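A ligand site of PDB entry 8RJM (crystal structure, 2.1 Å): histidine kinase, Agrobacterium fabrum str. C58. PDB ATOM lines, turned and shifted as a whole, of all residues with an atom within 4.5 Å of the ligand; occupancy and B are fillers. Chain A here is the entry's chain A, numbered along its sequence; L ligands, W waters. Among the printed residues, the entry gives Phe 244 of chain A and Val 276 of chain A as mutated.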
ATOM      1  N   LEU A  10      -6.792 -15.827  11.320  1.00  0.00           N
ATOM      2  CA  LEU A  10      -7.636 -15.962  10.100  1.00  0.00           C
ATOM      3  C   LEU A  10      -9.124 -15.796  10.434  1.00  0.00           C
ATOM      4  O   LEU A  10      -9.928 -15.752   9.479  1.00  0.00           O
ATOM      5  CB  LEU A  10      -7.376 -17.330   9.454  1.00  0.00           C
ATOM      6  CG  LEU A  10      -5.944 -17.573   8.963  1.00  0.00           C
ATOM      7  CD1 LEU A  10      -5.773 -19.012   8.516  1.00  0.00           C
ATOM      8  CD2 LEU A  10      -5.579 -16.626   7.831  1.00  0.00           C
ATOM      9  N   CYS A  13      -9.104 -11.281  11.137  1.00  0.00           N
ATOM     10  CA  CYS A  13      -8.224 -10.391  10.319  1.00  0.00           C
ATOM     11  C   CYS A  13      -9.067  -9.496   9.382  1.00  0.00           C
ATOM     12  O   CYS A  13      -8.519  -8.479   8.909  1.00  0.00           O
ATOM     13  CB  CYS A  13      -7.192 -11.185   9.526  1.00  0.00           C
ATOM     14  SG  CYS A  13      -7.891 -12.218   8.219  1.00  0.00           S
ATOM     15  N   ASP A  14     -10.329  -9.854   9.152  1.00  0.00           N
ATOM     16  CA  ASP A  14     -11.310  -9.061   8.357  1.00  0.00           C
ATOM     17  C   ASP A  14     -11.683  -7.767   9.100  1.00  0.00           C
ATOM     18  O   ASP A  14     -12.218  -6.847   8.437  1.00  0.00           O
ATOM     19  CB  ASP A  14     -12.559  -9.875   8.030  1.00  0.00           C
ATOM     20  CG  ASP A  14     -13.397 -10.251   9.236  1.00  0.00           C
ATOM     21  OD1 ASP A  14     -12.820 -10.731  10.238  1.00  0.00           O
ATOM     22  OD2 ASP A  14     -14.631 -10.061   9.184  1.00  0.00           O
ATOM     23  N   ILE A  18      -5.960  -1.927  11.299  1.00  0.00           N
ATOM     24  CA  ILE A  18      -4.624  -1.760  10.649  1.00  0.00           C
ATOM     25  C   ILE A  18      -4.224  -0.277  10.632  1.00  0.00           C
ATOM     26  O   ILE A  18      -3.043  -0.001  10.355  1.00  0.00           O
ATOM     27  CB  ILE A  18      -4.613  -2.381   9.238  1.00  0.00           C
ATOM     28  CG1 ILE A  18      -5.669  -1.757   8.314  1.00  0.00           C
ATOM     29  CG2 ILE A  18      -4.767  -3.889   9.320  1.00  0.00           C
ATOM     30  CD1 ILE A  18      -5.411  -1.988   6.847  1.00  0.00           C
ATOM     31  N   TYR A 165      -3.958  -5.005 -10.699  1.00  0.00           N
ATOM     32  CA  TYR A 165      -5.233  -5.655 -10.270  1.00  0.00           C
ATOM     33  C   TYR A 165      -6.407  -4.755 -10.673  1.00  0.00           C
ATOM     34  O   TYR A 165      -6.333  -3.538 -10.427  1.00  0.00           O
ATOM     35  CB  TYR A 165      -5.286  -5.859  -8.752  1.00  0.00           C
ATOM     36  CG  TYR A 165      -4.085  -6.530  -8.135  1.00  0.00           C
ATOM     37  CD1 TYR A 165      -3.523  -7.666  -8.710  1.00  0.00           C
ATOM     38  CD2 TYR A 165      -3.532  -6.056  -6.967  1.00  0.00           C
ATOM     39  CE1 TYR A 165      -2.429  -8.293  -8.130  1.00  0.00           C
ATOM     40  CE2 TYR A 165      -2.443  -6.674  -6.377  1.00  0.00           C
ATOM     41  CZ  TYR A 165      -1.886  -7.790  -6.962  1.00  0.00           C
ATOM     42  OH  TYR A 165      -0.807  -8.401  -6.384  1.00  0.00           O
ATOM     43  N   PHE A 187       1.174 -14.708 -12.544  1.00  0.00           N
ATOM     44  CA  PHE A 187      -0.165 -14.598 -11.903  1.00  0.00           C
ATOM     45  C   PHE A 187      -1.184 -14.015 -12.893  1.00  0.00           C
ATOM     46  O   PHE A 187      -2.300 -13.676 -12.464  1.00  0.00           O
ATOM     47  CB  PHE A 187      -0.099 -13.737 -10.638  1.00  0.00           C
ATOM     48  CG  PHE A 187       0.821 -14.249  -9.555  1.00  0.00           C
ATOM     49  CD1 PHE A 187       0.718 -15.549  -9.098  1.00  0.00           C
ATOM     50  CD2 PHE A 187       1.764 -13.416  -8.978  1.00  0.00           C
ATOM     51  CE1 PHE A 187       1.542 -16.012  -8.090  1.00  0.00           C
ATOM     52  CE2 PHE A 187       2.603 -13.884  -7.976  1.00  0.00           C
ATOM     53  CZ  PHE A 187       2.490 -15.178  -7.532  1.00  0.00           C
ATOM     54  N   GLN A 190      -5.180 -14.627 -13.217  1.00  0.00           N
ATOM     55  CA  GLN A 190      -5.541 -15.206 -11.897  1.00  0.00           C
ATOM     56  C   GLN A 190      -6.451 -14.229 -11.150  1.00  0.00           C
ATOM     57  O   GLN A 190      -6.305 -13.003 -11.331  1.00  0.00           O
ATOM     58  CB  GLN A 190      -4.277 -15.498 -11.087  1.00  0.00           C
ATOM     59  CG  GLN A 190      -4.518 -16.408  -9.897  1.00  0.00           C
ATOM     60  CD  GLN A 190      -3.229 -16.919  -9.295  1.00  0.00           C
ATOM     61  OE1 GLN A 190      -2.278 -17.240 -10.008  1.00  0.00           O
ATOM     62  NE2 GLN A 190      -3.177 -17.003  -7.977  1.00  0.00           N
ATOM     63  N   PHE A 192      -8.214 -13.241  -7.151  1.00  0.00           N
ATOM     64  CA  PHE A 192      -8.199 -13.389  -5.672  1.00  0.00           C
ATOM     65  C   PHE A 192      -9.543 -12.930  -5.118  1.00  0.00           C
ATOM     66  O   PHE A 192     -10.179 -12.035  -5.675  1.00  0.00           O
ATOM     67  CB  PHE A 192      -6.988 -12.679  -5.052  1.00  0.00           C
ATOM     68  CG  PHE A 192      -6.859 -11.194  -5.278  1.00  0.00           C
ATOM     69  CD1 PHE A 192      -7.627 -10.293  -4.540  1.00  0.00           C
ATOM     70  CD2 PHE A 192      -5.935 -10.685  -6.169  1.00  0.00           C
ATOM     71  CE1 PHE A 192      -7.494  -8.933  -4.734  1.00  0.00           C
ATOM     72  CE2 PHE A 192      -5.799  -9.314  -6.350  1.00  0.00           C
ATOM     73  CZ  PHE A 192      -6.584  -8.440  -5.629  1.00  0.00           C
ATOM     74  N   SER A 195     -12.042 -10.995   0.225  1.00  0.00           N
ATOM     75  CA  SER A 195     -11.549 -11.137   1.628  1.00  0.00           C
ATOM     76  C   SER A 195     -10.023 -10.971   1.706  1.00  0.00           C
ATOM     77  O   SER A 195      -9.535 -10.619   2.805  1.00  0.00           O
ATOM     78  CB  SER A 195     -11.966 -12.466   2.204  1.00  0.00           C
ATOM     79  OG  SER A 195     -11.459 -13.541   1.442  1.00  0.00           O
ATOM     80  N   ASP A 196      -9.292 -11.200   0.618  1.00  0.00           N
ATOM     81  CA  ASP A 196      -7.808 -11.084   0.566  1.00  0.00           C
ATOM     82  C   ASP A 196      -7.369  -9.625   0.777  1.00  0.00           C
ATOM     83  O   ASP A 196      -6.197  -9.426   1.135  1.00  0.00           O
ATOM     84  CB  ASP A 196      -7.236 -11.622  -0.747  1.00  0.00           C
ATOM     85  CG  ASP A 196      -6.970 -13.124  -0.736  1.00  0.00           C
ATOM     86  OD1 ASP A 196      -7.496 -13.805   0.155  1.00  0.00           O
ATOM     87  OD2 ASP A 196      -6.236 -13.582  -1.624  1.00  0.00           O
ATOM     88  N   ILE A 197      -8.260  -8.660   0.530  1.00  0.00           N
ATOM     89  CA  ILE A 197      -8.045  -7.217   0.875  1.00  0.00           C
ATOM     90  C   ILE A 197      -9.250  -6.744   1.687  1.00  0.00           C
ATOM     91  O   ILE A 197     -10.290  -6.417   1.117  1.00  0.00           O
ATOM     92  CB  ILE A 197      -7.810  -6.353  -0.383  1.00  0.00           C
ATOM     93  CG1 ILE A 197      -6.675  -6.907  -1.262  1.00  0.00           C
ATOM     94  CG2 ILE A 197      -7.564  -4.908   0.002  1.00  0.00           C
ATOM     95  CD1 ILE A 197      -6.491  -6.169  -2.565  1.00  0.00           C
ATOM     96  N   PRO A 198      -9.148  -6.723   3.037  1.00  0.00           N
ATOM     97  CA  PRO A 198     -10.248  -6.274   3.897  1.00  0.00           C
ATOM     98  C   PRO A 198     -10.718  -4.832   3.607  1.00  0.00           C
ATOM     99  O   PRO A 198      -9.980  -4.099   2.976  1.00  0.00           O
ATOM    100  CB  PRO A 198      -9.668  -6.339   5.319  1.00  0.00           C
ATOM    101  CG  PRO A 198      -8.525  -7.335   5.217  1.00  0.00           C
ATOM    102  CD  PRO A 198      -7.975  -7.156   3.812  1.00  0.00           C
ATOM    103  N   ALA A 201      -8.492  -1.920   4.688  1.00  0.00           N
ATOM    104  CA  ALA A 201      -7.347  -1.831   3.740  1.00  0.00           C
ATOM    105  C   ALA A 201      -7.766  -1.061   2.482  1.00  0.00           C
ATOM    106  O   ALA A 201      -6.992  -0.193   2.038  1.00  0.00           O
ATOM    107  CB  ALA A 201      -6.825  -3.201   3.405  1.00  0.00           C
ATOM    108  N   TYR A 205      -6.237   2.481   0.980  1.00  0.00           N
ATOM    109  CA  TYR A 205      -5.801   2.510  -0.448  1.00  0.00           C
ATOM    110  C   TYR A 205      -6.471   3.698  -1.147  1.00  0.00           C
ATOM    111  O   TYR A 205      -5.860   4.282  -2.054  1.00  0.00           O
ATOM    112  CB  TYR A 205      -6.096   1.190  -1.158  1.00  0.00           C
ATOM    113  CG  TYR A 205      -5.143   0.057  -0.867  1.00  0.00           C
ATOM    114  CD1 TYR A 205      -3.772   0.236  -0.955  1.00  0.00           C
ATOM    115  CD2 TYR A 205      -5.606  -1.209  -0.548  1.00  0.00           C
ATOM    116  CE1 TYR A 205      -2.879  -0.803  -0.693  1.00  0.00           C
ATOM    117  CE2 TYR A 205      -4.732  -2.255  -0.291  1.00  0.00           C
ATOM    118  CZ  TYR A 205      -3.361  -2.055  -0.367  1.00  0.00           C
ATOM    119  OH  TYR A 205      -2.485  -3.068  -0.118  1.00  0.00           O
ATOM    120  N   ARG A 211       1.448   3.177  -0.976  1.00  0.00           N
ATOM    121  CA  ARG A 211       1.640   2.322   0.222  1.00  0.00           C
ATOM    122  C   ARG A 211       2.973   1.588   0.048  1.00  0.00           C
ATOM    123  O   ARG A 211       3.161   0.934  -0.995  1.00  0.00           O
ATOM    124  CB  ARG A 211       0.437   1.374   0.386  1.00  0.00           C
ATOM    125  CG  ARG A 211       0.617   0.287   1.437  1.00  0.00           C
ATOM    126  CD  ARG A 211       1.034   0.831   2.782  1.00  0.00           C
ATOM    127  NE  ARG A 211       0.910  -0.145   3.853  1.00  0.00           N
ATOM    128  CZ  ARG A 211       1.400   0.008   5.082  1.00  0.00           C
ATOM    129  NH1 ARG A 211       2.064   1.106   5.407  1.00  0.00           N
ATOM    130  NH2 ARG A 211       1.230  -0.945   5.986  1.00  0.00           N
ATOM    131  N   ILE A 213       5.984  -1.003   1.708  1.00  0.00           N
ATOM    132  CA  ILE A 213       6.569  -1.994   2.660  1.00  0.00           C
ATOM    133  C   ILE A 213       8.042  -2.167   2.279  1.00  0.00           C
ATOM    134  O   ILE A 213       8.311  -2.802   1.239  1.00  0.00           O
ATOM    135  CB  ILE A 213       5.781  -3.314   2.656  1.00  0.00           C
ATOM    136  CG1 ILE A 213       4.312  -3.096   3.042  1.00  0.00           C
ATOM    137  CG2 ILE A 213       6.454  -4.348   3.556  1.00  0.00           C
ATOM    138  CD1 ILE A 213       3.442  -4.320   2.931  1.00  0.00           C
ATOM    139  N   ARG A 242       3.675   3.808   8.611  1.00  0.00           N
ATOM    140  CA  ARG A 242       2.715   2.907   9.303  1.00  0.00           C
ATOM    141  C   ARG A 242       3.094   1.442   9.045  1.00  0.00           C
ATOM    142  O   ARG A 242       3.308   1.084   7.878  1.00  0.00           O
ATOM    143  CB  ARG A 242       1.283   3.186   8.840  1.00  0.00           C
ATOM    144  CG  ARG A 242       0.236   2.240   9.400  1.00  0.00           C
ATOM    145  CD  ARG A 242      -1.166   2.594   8.963  1.00  0.00           C
ATOM    146  NE  ARG A 242      -1.258   2.714   7.512  1.00  0.00           N
ATOM    147  CZ  ARG A 242      -1.500   1.710   6.676  1.00  0.00           C
ATOM    148  NH1 ARG A 242      -1.544   1.936   5.372  1.00  0.00           N
ATOM    149  NH2 ARG A 242      -1.710   0.488   7.130  1.00  0.00           N
ATOM    150  N   PHE A 244       2.646  -2.786   8.842  1.00  0.00           N
ATOM    151  CA  PHE A 244       1.723  -3.637   8.040  1.00  0.00           C
ATOM    152  C   PHE A 244       1.248  -4.812   8.904  1.00  0.00           C
ATOM    153  O   PHE A 244       1.954  -5.203   9.845  1.00  0.00           O
ATOM    154  CB  PHE A 244       2.416  -4.107   6.755  1.00  0.00           C
ATOM    155  CG  PHE A 244       3.817  -4.616   6.951  1.00  0.00           C
ATOM    156  CD1 PHE A 244       4.893  -3.743   7.006  1.00  0.00           C
ATOM    157  CD2 PHE A 244       4.071  -5.981   7.084  1.00  0.00           C
ATOM    158  CE1 PHE A 244       6.180  -4.210   7.195  1.00  0.00           C
ATOM    159  CE2 PHE A 244       5.361  -6.446   7.263  1.00  0.00           C
ATOM    160  CZ  PHE A 244       6.418  -5.559   7.325  1.00  0.00           C
ATOM    161  N   SER A 245       0.083  -5.370   8.570  1.00  0.00           N
ATOM    162  CA  SER A 245      -0.569  -6.508   9.275  1.00  0.00           C
ATOM    163  C   SER A 245       0.343  -7.737   9.235  1.00  0.00           C
ATOM    164  O   SER A 245       0.901  -8.050   8.197  1.00  0.00           O
ATOM    165  CB  SER A 245      -1.925  -6.822   8.679  1.00  0.00           C
ATOM    166  OG  SER A 245      -2.392  -8.088   9.122  1.00  0.00           O
ATOM    167  N   ILE A 247      -0.616 -10.681   9.112  1.00  0.00           N
ATOM    168  CA  ILE A 247      -1.326 -11.605   8.175  1.00  0.00           C
ATOM    169  C   ILE A 247      -0.749 -11.406   6.769  1.00  0.00           C
ATOM    170  O   ILE A 247      -0.375 -12.409   6.133  1.00  0.00           O
ATOM    171  CB  ILE A 247      -2.846 -11.381   8.214  1.00  0.00           C
ATOM    172  CG1 ILE A 247      -3.423 -11.580   9.621  1.00  0.00           C
ATOM    173  CG2 ILE A 247      -3.555 -12.263   7.188  1.00  0.00           C
ATOM    174  CD1 ILE A 247      -3.257 -12.970  10.185  1.00  0.00           C
ATOM    175  N   HIS A 248      -0.662 -10.154   6.314  1.00  0.00           N
ATOM    176  CA  HIS A 248      -0.106  -9.790   4.989  1.00  0.00           C
ATOM    177  C   HIS A 248       1.403 -10.082   4.962  1.00  0.00           C
ATOM    178  O   HIS A 248       1.881 -10.606   3.936  1.00  0.00           O
ATOM    179  CB  HIS A 248      -0.389  -8.334   4.616  1.00  0.00           C
ATOM    180  CG  HIS A 248       0.046  -8.006   3.223  1.00  0.00           C
ATOM    181  ND1 HIS A 248      -0.427  -8.694   2.131  1.00  0.00           N
ATOM    182  CD2 HIS A 248       0.920  -7.091   2.758  1.00  0.00           C
ATOM    183  CE1 HIS A 248       0.134  -8.207   1.036  1.00  0.00           C
ATOM    184  NE2 HIS A 248       0.965  -7.228   1.397  1.00  0.00           N
ATOM    185  N   TYR A 251       1.905 -13.612   4.275  1.00  0.00           N
ATOM    186  CA  TYR A 251       1.500 -13.833   2.856  1.00  0.00           C
ATOM    187  C   TYR A 251       2.697 -13.553   1.938  1.00  0.00           C
ATOM    188  O   TYR A 251       3.001 -14.395   1.078  1.00  0.00           O
ATOM    189  CB  TYR A 251       0.283 -12.981   2.469  1.00  0.00           C
ATOM    190  CG  TYR A 251      -0.518 -13.558   1.328  1.00  0.00           C
ATOM    191  CD1 TYR A 251       0.004 -13.612   0.051  1.00  0.00           C
ATOM    192  CD2 TYR A 251      -1.786 -14.081   1.540  1.00  0.00           C
ATOM    193  CE1 TYR A 251      -0.714 -14.157  -1.002  1.00  0.00           C
ATOM    194  CE2 TYR A 251      -2.515 -14.630   0.494  1.00  0.00           C
ATOM    195  CZ  TYR A 251      -1.979 -14.667  -0.777  1.00  0.00           C
ATOM    196  OH  TYR A 251      -2.693 -15.210  -1.808  1.00  0.00           O
ATOM    197  N   MET A 255       5.351 -16.035  -0.464  1.00  0.00           N
ATOM    198  CA  MET A 255       5.526 -15.763  -1.923  1.00  0.00           C
ATOM    199  C   MET A 255       7.010 -15.536  -2.256  1.00  0.00           C
ATOM    200  O   MET A 255       7.346 -15.572  -3.457  1.00  0.00           O
ATOM    201  CB  MET A 255       4.741 -14.516  -2.356  1.00  0.00           C
ATOM    202  CG  MET A 255       3.244 -14.712  -2.346  1.00  0.00           C
ATOM    203  SD  MET A 255       2.368 -13.167  -2.707  1.00  0.00           S
ATOM    204  CE  MET A 255       2.799 -12.943  -4.432  1.00  0.00           C
ATOM    205  N   LEU A 274      -5.254  -1.536  -8.321  1.00  0.00           N
ATOM    206  CA  LEU A 274      -3.902  -1.203  -7.809  1.00  0.00           C
ATOM    207  C   LEU A 274      -2.857  -1.506  -8.889  1.00  0.00           C
ATOM    208  O   LEU A 274      -3.012  -2.528  -9.589  1.00  0.00           O
ATOM    209  CB  LEU A 274      -3.607  -2.030  -6.548  1.00  0.00           C
ATOM    210  CG  LEU A 274      -4.577  -1.825  -5.372  1.00  0.00           C
ATOM    211  CD1 LEU A 274      -4.299  -2.853  -4.279  1.00  0.00           C
ATOM    212  CD2 LEU A 274      -4.468  -0.418  -4.820  1.00  0.00           C
ATOM    213  N   VAL A 276       0.753  -2.712  -8.396  1.00  0.00           N
ATOM    214  CA  VAL A 276       1.544  -3.292  -7.281  1.00  0.00           C
ATOM    215  C   VAL A 276       2.921  -3.716  -7.803  1.00  0.00           C
ATOM    216  O   VAL A 276       2.981  -4.513  -8.757  1.00  0.00           O
ATOM    217  CB  VAL A 276       0.803  -4.463  -6.604  1.00  0.00           C
ATOM    218  CG1 VAL A 276       1.691  -5.201  -5.611  1.00  0.00           C
ATOM    219  CG2 VAL A 276      -0.462  -3.972  -5.911  1.00  0.00           C
ATOM    220  N   HIS A 278       6.324  -5.690  -6.588  1.00  0.00           N
ATOM    221  CA  HIS A 278       6.907  -6.682  -5.626  1.00  0.00           C
ATOM    222  C   HIS A 278       8.411  -6.808  -5.880  1.00  0.00           C
ATOM    223  O   HIS A 278       8.814  -6.830  -7.061  1.00  0.00           O
ATOM    224  CB  HIS A 278       6.225  -8.048  -5.739  1.00  0.00           C
ATOM    225  CG  HIS A 278       4.857  -8.110  -5.152  1.00  0.00           C
ATOM    226  ND1 HIS A 278       4.021  -9.195  -5.367  1.00  0.00           N
ATOM    227  CD2 HIS A 278       4.170  -7.242  -4.384  1.00  0.00           C
ATOM    228  CE1 HIS A 278       2.883  -8.989  -4.736  1.00  0.00           C
ATOM    229  NE2 HIS A 278       2.945  -7.801  -4.121  1.00  0.00           N
ATOM    230  N   ARG A 456      -3.668 -21.042   3.670  1.00  0.00           N
ATOM    231  CA  ARG A 456      -4.658 -19.976   3.332  1.00  0.00           C
ATOM    232  C   ARG A 456      -3.937 -18.758   2.736  1.00  0.00           C
ATOM    233  O   ARG A 456      -4.512 -18.125   1.830  1.00  0.00           O
ATOM    234  CB  ARG A 456      -5.486 -19.568   4.554  1.00  0.00           C
ATOM    235  CG  ARG A 456      -6.398 -18.365   4.331  1.00  0.00           C
ATOM    236  CD  ARG A 456      -7.430 -18.568   3.231  1.00  0.00           C
ATOM    237  NE  ARG A 456      -8.267 -17.401   2.994  1.00  0.00           N
ATOM    238  CZ  ARG A 456      -7.988 -16.406   2.155  1.00  0.00           C
ATOM    239  NH1 ARG A 456      -6.872 -16.398   1.442  1.00  0.00           N
ATOM    240  NH2 ARG A 456      -8.838 -15.402   2.016  1.00  0.00           N
ATOM    241  N   LEU A 457      -2.733 -18.437   3.238  1.00  0.00           N
ATOM    242  CA  LEU A 457      -1.955 -17.237   2.844  1.00  0.00           C
ATOM    243  C   LEU A 457      -0.988 -17.581   1.707  1.00  0.00           C
ATOM    244  O   LEU A 457       0.215 -17.278   1.833  1.00  0.00           O
ATOM    245  CB  LEU A 457      -1.213 -16.691   4.070  1.00  0.00           C
ATOM    246  CG  LEU A 457      -2.092 -16.419   5.298  1.00  0.00           C
ATOM    247  CD1 LEU A 457      -1.250 -15.869   6.448  1.00  0.00           C
ATOM    248  CD2 LEU A 457      -3.221 -15.459   4.964  1.00  0.00           C
ATOM    249  N   PRO A 459      -0.983 -17.679  -2.960  1.00  0.00           N
ATOM    250  CA  PRO A 459      -1.728 -17.447  -4.195  1.00  0.00           C
ATOM    251  C   PRO A 459      -2.554 -18.660  -4.647  1.00  0.00           C
ATOM    252  O   PRO A 459      -3.670 -18.477  -5.114  1.00  0.00           O
ATOM    253  CB  PRO A 459      -0.620 -17.159  -5.230  1.00  0.00           C
ATOM    254  CG  PRO A 459       0.514 -16.592  -4.404  1.00  0.00           C
ATOM    255  CD  PRO A 459       0.433 -17.323  -3.083  1.00  0.00           C
ATOM    256  N   SER A 462      -5.702 -18.885  -2.397  1.00  0.00           N
ATOM    257  CA  SER A 462      -6.495 -17.661  -2.741  1.00  0.00           C
ATOM    258  C   SER A 462      -7.342 -17.937  -3.995  1.00  0.00           C
ATOM    259  O   SER A 462      -8.570 -17.700  -3.947  1.00  0.00           O
ATOM    260  CB  SER A 462      -5.613 -16.449  -2.909  1.00  0.00           C
ATOM    261  OG  SER A 462      -5.280 -15.873  -1.657  1.00  0.00           O
HETATM  262  C1  LIG L   1      -5.305 -12.266   3.234  1.00  0.00           C
HETATM  263  C2  LIG L   1      -4.602  -8.017   4.071  1.00  0.00           C
HETATM  264  O1  LIG L   1      -0.468  -2.556   2.911  1.00  0.00           O
HETATM  265  C3  LIG L   1      -3.029  -7.570   0.077  1.00  0.00           C
HETATM  266  O2  LIG L   1       0.950  -6.648  -2.626  1.00  0.00           O
HETATM  267  C4  LIG L   1      -3.003 -11.341  -2.830  1.00  0.00           C
HETATM  268  C5  LIG L   1      -6.241 -12.383   4.258  1.00  0.00           C
HETATM  269  C6  LIG L   1      -4.258  -6.758   4.551  1.00  0.00           C
HETATM  270  O3  LIG L   1      -0.891  -2.887   5.035  1.00  0.00           O
HETATM  271  C7  LIG L   1      -2.864  -7.171  -1.249  1.00  0.00           C
HETATM  272  O4  LIG L   1      -0.832  -6.729  -3.901  1.00  0.00           O
HETATM  273  C8  LIG L   1      -1.744 -11.278  -3.426  1.00  0.00           C
HETATM  274  C9  LIG L   1      -6.350 -11.234   5.010  1.00  0.00           C
HETATM  275  C10 LIG L   1      -3.567  -6.114   3.525  1.00  0.00           C
HETATM  276  C11 LIG L   1      -3.153  -8.255  -2.053  1.00  0.00           C
HETATM  277  C12 LIG L   1      -1.654 -12.340  -4.333  1.00  0.00           C
HETATM  278  C13 LIG L   1      -5.522 -10.318   4.366  1.00  0.00           C
HETATM  279  C14 LIG L   1      -3.574  -6.981   2.441  1.00  0.00           C
HETATM  280  C15 LIG L   1      -3.450  -9.354  -1.248  1.00  0.00           C
HETATM  281  C16 LIG L   1      -2.835 -13.068  -4.259  1.00  0.00           C
HETATM  282  C17 LIG L   1      -7.231 -11.009   6.087  1.00  0.00           C
HETATM  283  C18 LIG L   1      -2.967  -4.736   3.564  1.00  0.00           C
HETATM  284  C19 LIG L   1      -2.476  -5.807  -1.737  1.00  0.00           C
HETATM  285  C20 LIG L   1      -0.598 -12.592  -5.219  1.00  0.00           C
HETATM  286  C21 LIG L   1      -8.090 -11.897   6.579  1.00  0.00           C
HETATM  287  C22 LIG L   1      -1.435  -4.645   3.534  1.00  0.00           C
HETATM  288  C23 LIG L   1      -0.983  -5.529  -1.835  1.00  0.00           C
HETATM  289  C24 LIG L   1      -0.685 -13.108  -6.440  1.00  0.00           C
HETATM  290  C25 LIG L   1      -0.901  -3.255   3.848  1.00  0.00           C
HETATM  291  C26 LIG L   1      -0.242  -6.361  -2.866  1.00  0.00           C
HETATM  292  C27 LIG L   1      -5.370  -8.985   4.727  1.00  0.00           C
HETATM  293  C28 LIG L   1      -2.943  -6.779   1.217  1.00  0.00           C
HETATM  294  C29 LIG L   1      -3.703 -10.560  -1.906  1.00  0.00           C
HETATM  295  C30 LIG L   1      -6.594 -13.742   4.807  1.00  0.00           C
HETATM  296  C31 LIG L   1      -4.517  -6.209   5.919  1.00  0.00           C
HETATM  297  C32 LIG L   1      -3.108  -8.256  -3.549  1.00  0.00           C
HETATM  298  C33 LIG L   1      -0.615 -10.307  -3.193  1.00  0.00           C
HETATM  299  N1  LIG L   1      -4.879 -10.953   3.304  1.00  0.00           N
HETATM  300  O5  LIG L   1      -4.938 -13.105   2.454  1.00  0.00           O
HETATM  301  N2  LIG L   1      -4.249  -8.123   2.755  1.00  0.00           N
HETATM  302  N3  LIG L   1      -3.475  -8.890   0.043  1.00  0.00           N
HETATM  303  N4  LIG L   1      -3.648 -12.457  -3.339  1.00  0.00           N
HETATM  304  O6  LIG L   1      -3.148 -14.083  -4.887  1.00  0.00           O
HETATM  305  O   HOH W   1     -11.202 -12.748   6.062  1.00  0.00           O
HETATM  306  O   HOH W   2      -2.305 -10.614   2.030  1.00  0.00           O
HETATM  307  O   HOH W   3       1.950  -5.187  -0.431  1.00  0.00           O
HETATM  308  O   HOH W   4      -4.914 -15.425  -6.543  1.00  0.00           O
HETATM  309  O   HOH W   5      -2.612  -0.663   4.739  1.00  0.00           O
HETATM  310  O   HOH W   6      -1.757  -3.734   7.245  1.00  0.00           O
HETATM  311  O   HOH W   7       0.287  -3.189   0.278  1.00  0.00           O
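A nitrogen (N4) of the ligand sits at hydrogen-bond distance from the side-chain carboxylate (OD2) of Asp 196, 3.3 Å away. N4 of the ligand sits close to OH of Tyr 251 (3.3 Å). The backbone carbonyl oxygen of Asp 196 lies within hydrogen-bond range of a nitrogen (N1) of the ligand. O1 of the ligand is in salt-bridge range of NE of Arg 211 (2.9 Å). A carbon (C21) of the ligand is bonded to the side-chain sulfur of Cys 13. NE2 of His 278 is in hydrogen-bond range of O2 of the ligand. The side-chain hydroxyl of Tyr 165 lies close to an oxygen (O4) of the ligand, at 3.0 Å.
The side-chain hydroxyl of Ser 462 sits at hydrogen-bond distance from the side-chain carboxylate of Asp 196, 2.5 Å away. OG of Ser 462 is in hydrogen-bond range of OH of Tyr 251 (2.7 Å). O of Pro 459 sits at hydrogen-bond distance from NE2 of Gln 190 (3.3 Å). NH1 of Arg 211 is in hydrogen-bond range of O of Arg 242, 2.8 Å away. The guanidinium group of Arg 456 is in salt-bridge range of the side-chain carboxylate of Asp 196 (2.8 Å). The side-chain hydroxyl (OG) of Ser 195 lies within hydrogen-bond range of the guanidinium group (NH2) of Arg 456. The backbone NH of Ile 247 sits close to the side-chain hydroxyl of Ser 245. The backbone NH (N) of Tyr 165 sits at hydrogen-bond distance from the backbone carbonyl oxygen (O) of Leu 274, 2.9 Å away.
Asp 14 touches the ligand (N to C21, 3.98 Å). CD2 of Phe 187 touches C24 of the ligand (3.5 Å). Phe 192 touches the ligand (CB to N4, 3.8 Å). Ser 195 touches the ligand. CG1 of Ile 197 touches C7 of the ligand, at 3.8 Å. Pro 198 touches the ligand (CD to C27, 3.3 Å). Tyr 205 touches the ligand. CB of Phe 244 touches O3 of the ligand (3.9 Å). CB of Ser 245 touches C31 of the ligand, at 3.8 Å. Ile 247 touches the ligand. His 248 touches the ligand. Met 255 touches the ligand (CE to C20, 3.5 Å). Val 276 touches the ligand (CG1 to O2, 3.4 Å). Arg 456 touches the ligand (NH2 to C30, 3.9 Å). Leu 457 touches the ligand. Pro 459 touches the ligand. Ser 462 touches the ligand. Hydrophobic or aromatic side chains within 4 Å of the ligand: Tyr 165, Phe 187, Phe 192, Ile 197, Pro 198, Phe 244, Ile 247, His 248, Tyr 251, Met 255, Val 276, His 278, Leu 457 and Pro 459. Within 4 Å of the ligand: Cys 13, Asp 14, Tyr 165, Phe 187, Phe 192, Ser 195, Asp 196, Ile 197, Pro 198, Tyr 205, Arg 211, Phe 244, Ser 245, Ile 247, His 248, Tyr 251, Met 255, Val 276, His 278, Arg 456, Leu 457, Pro 459 and Ser 462.
Water W6 lies within hydrogen-bond range of O3 of the ligand (2.5 Å) and N of Ser 245 (2.8 Å). Water W4 bridges NE2 of Gln 190 (2.8 Å) and O6 of the ligand (2.8 Å). Water W7 lies within hydrogen-bond range of OH of Tyr 205 (2.8 Å) and O1 of the ligand (2.8 Å). Water W3 lies within hydrogen-bond range of an oxygen (O2) of the ligand (2.8 Å) and a ring nitrogen (NE2) of His 248 (2.9 Å). Water W5 lies within hydrogen-bond range of NH2 of Arg 242 (2.8 Å) and O3 of the ligand (2.8 Å). Water W2 bridges ND1 of His 248 (2.7 Å) and N3 of the ligand (2.9 Å).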
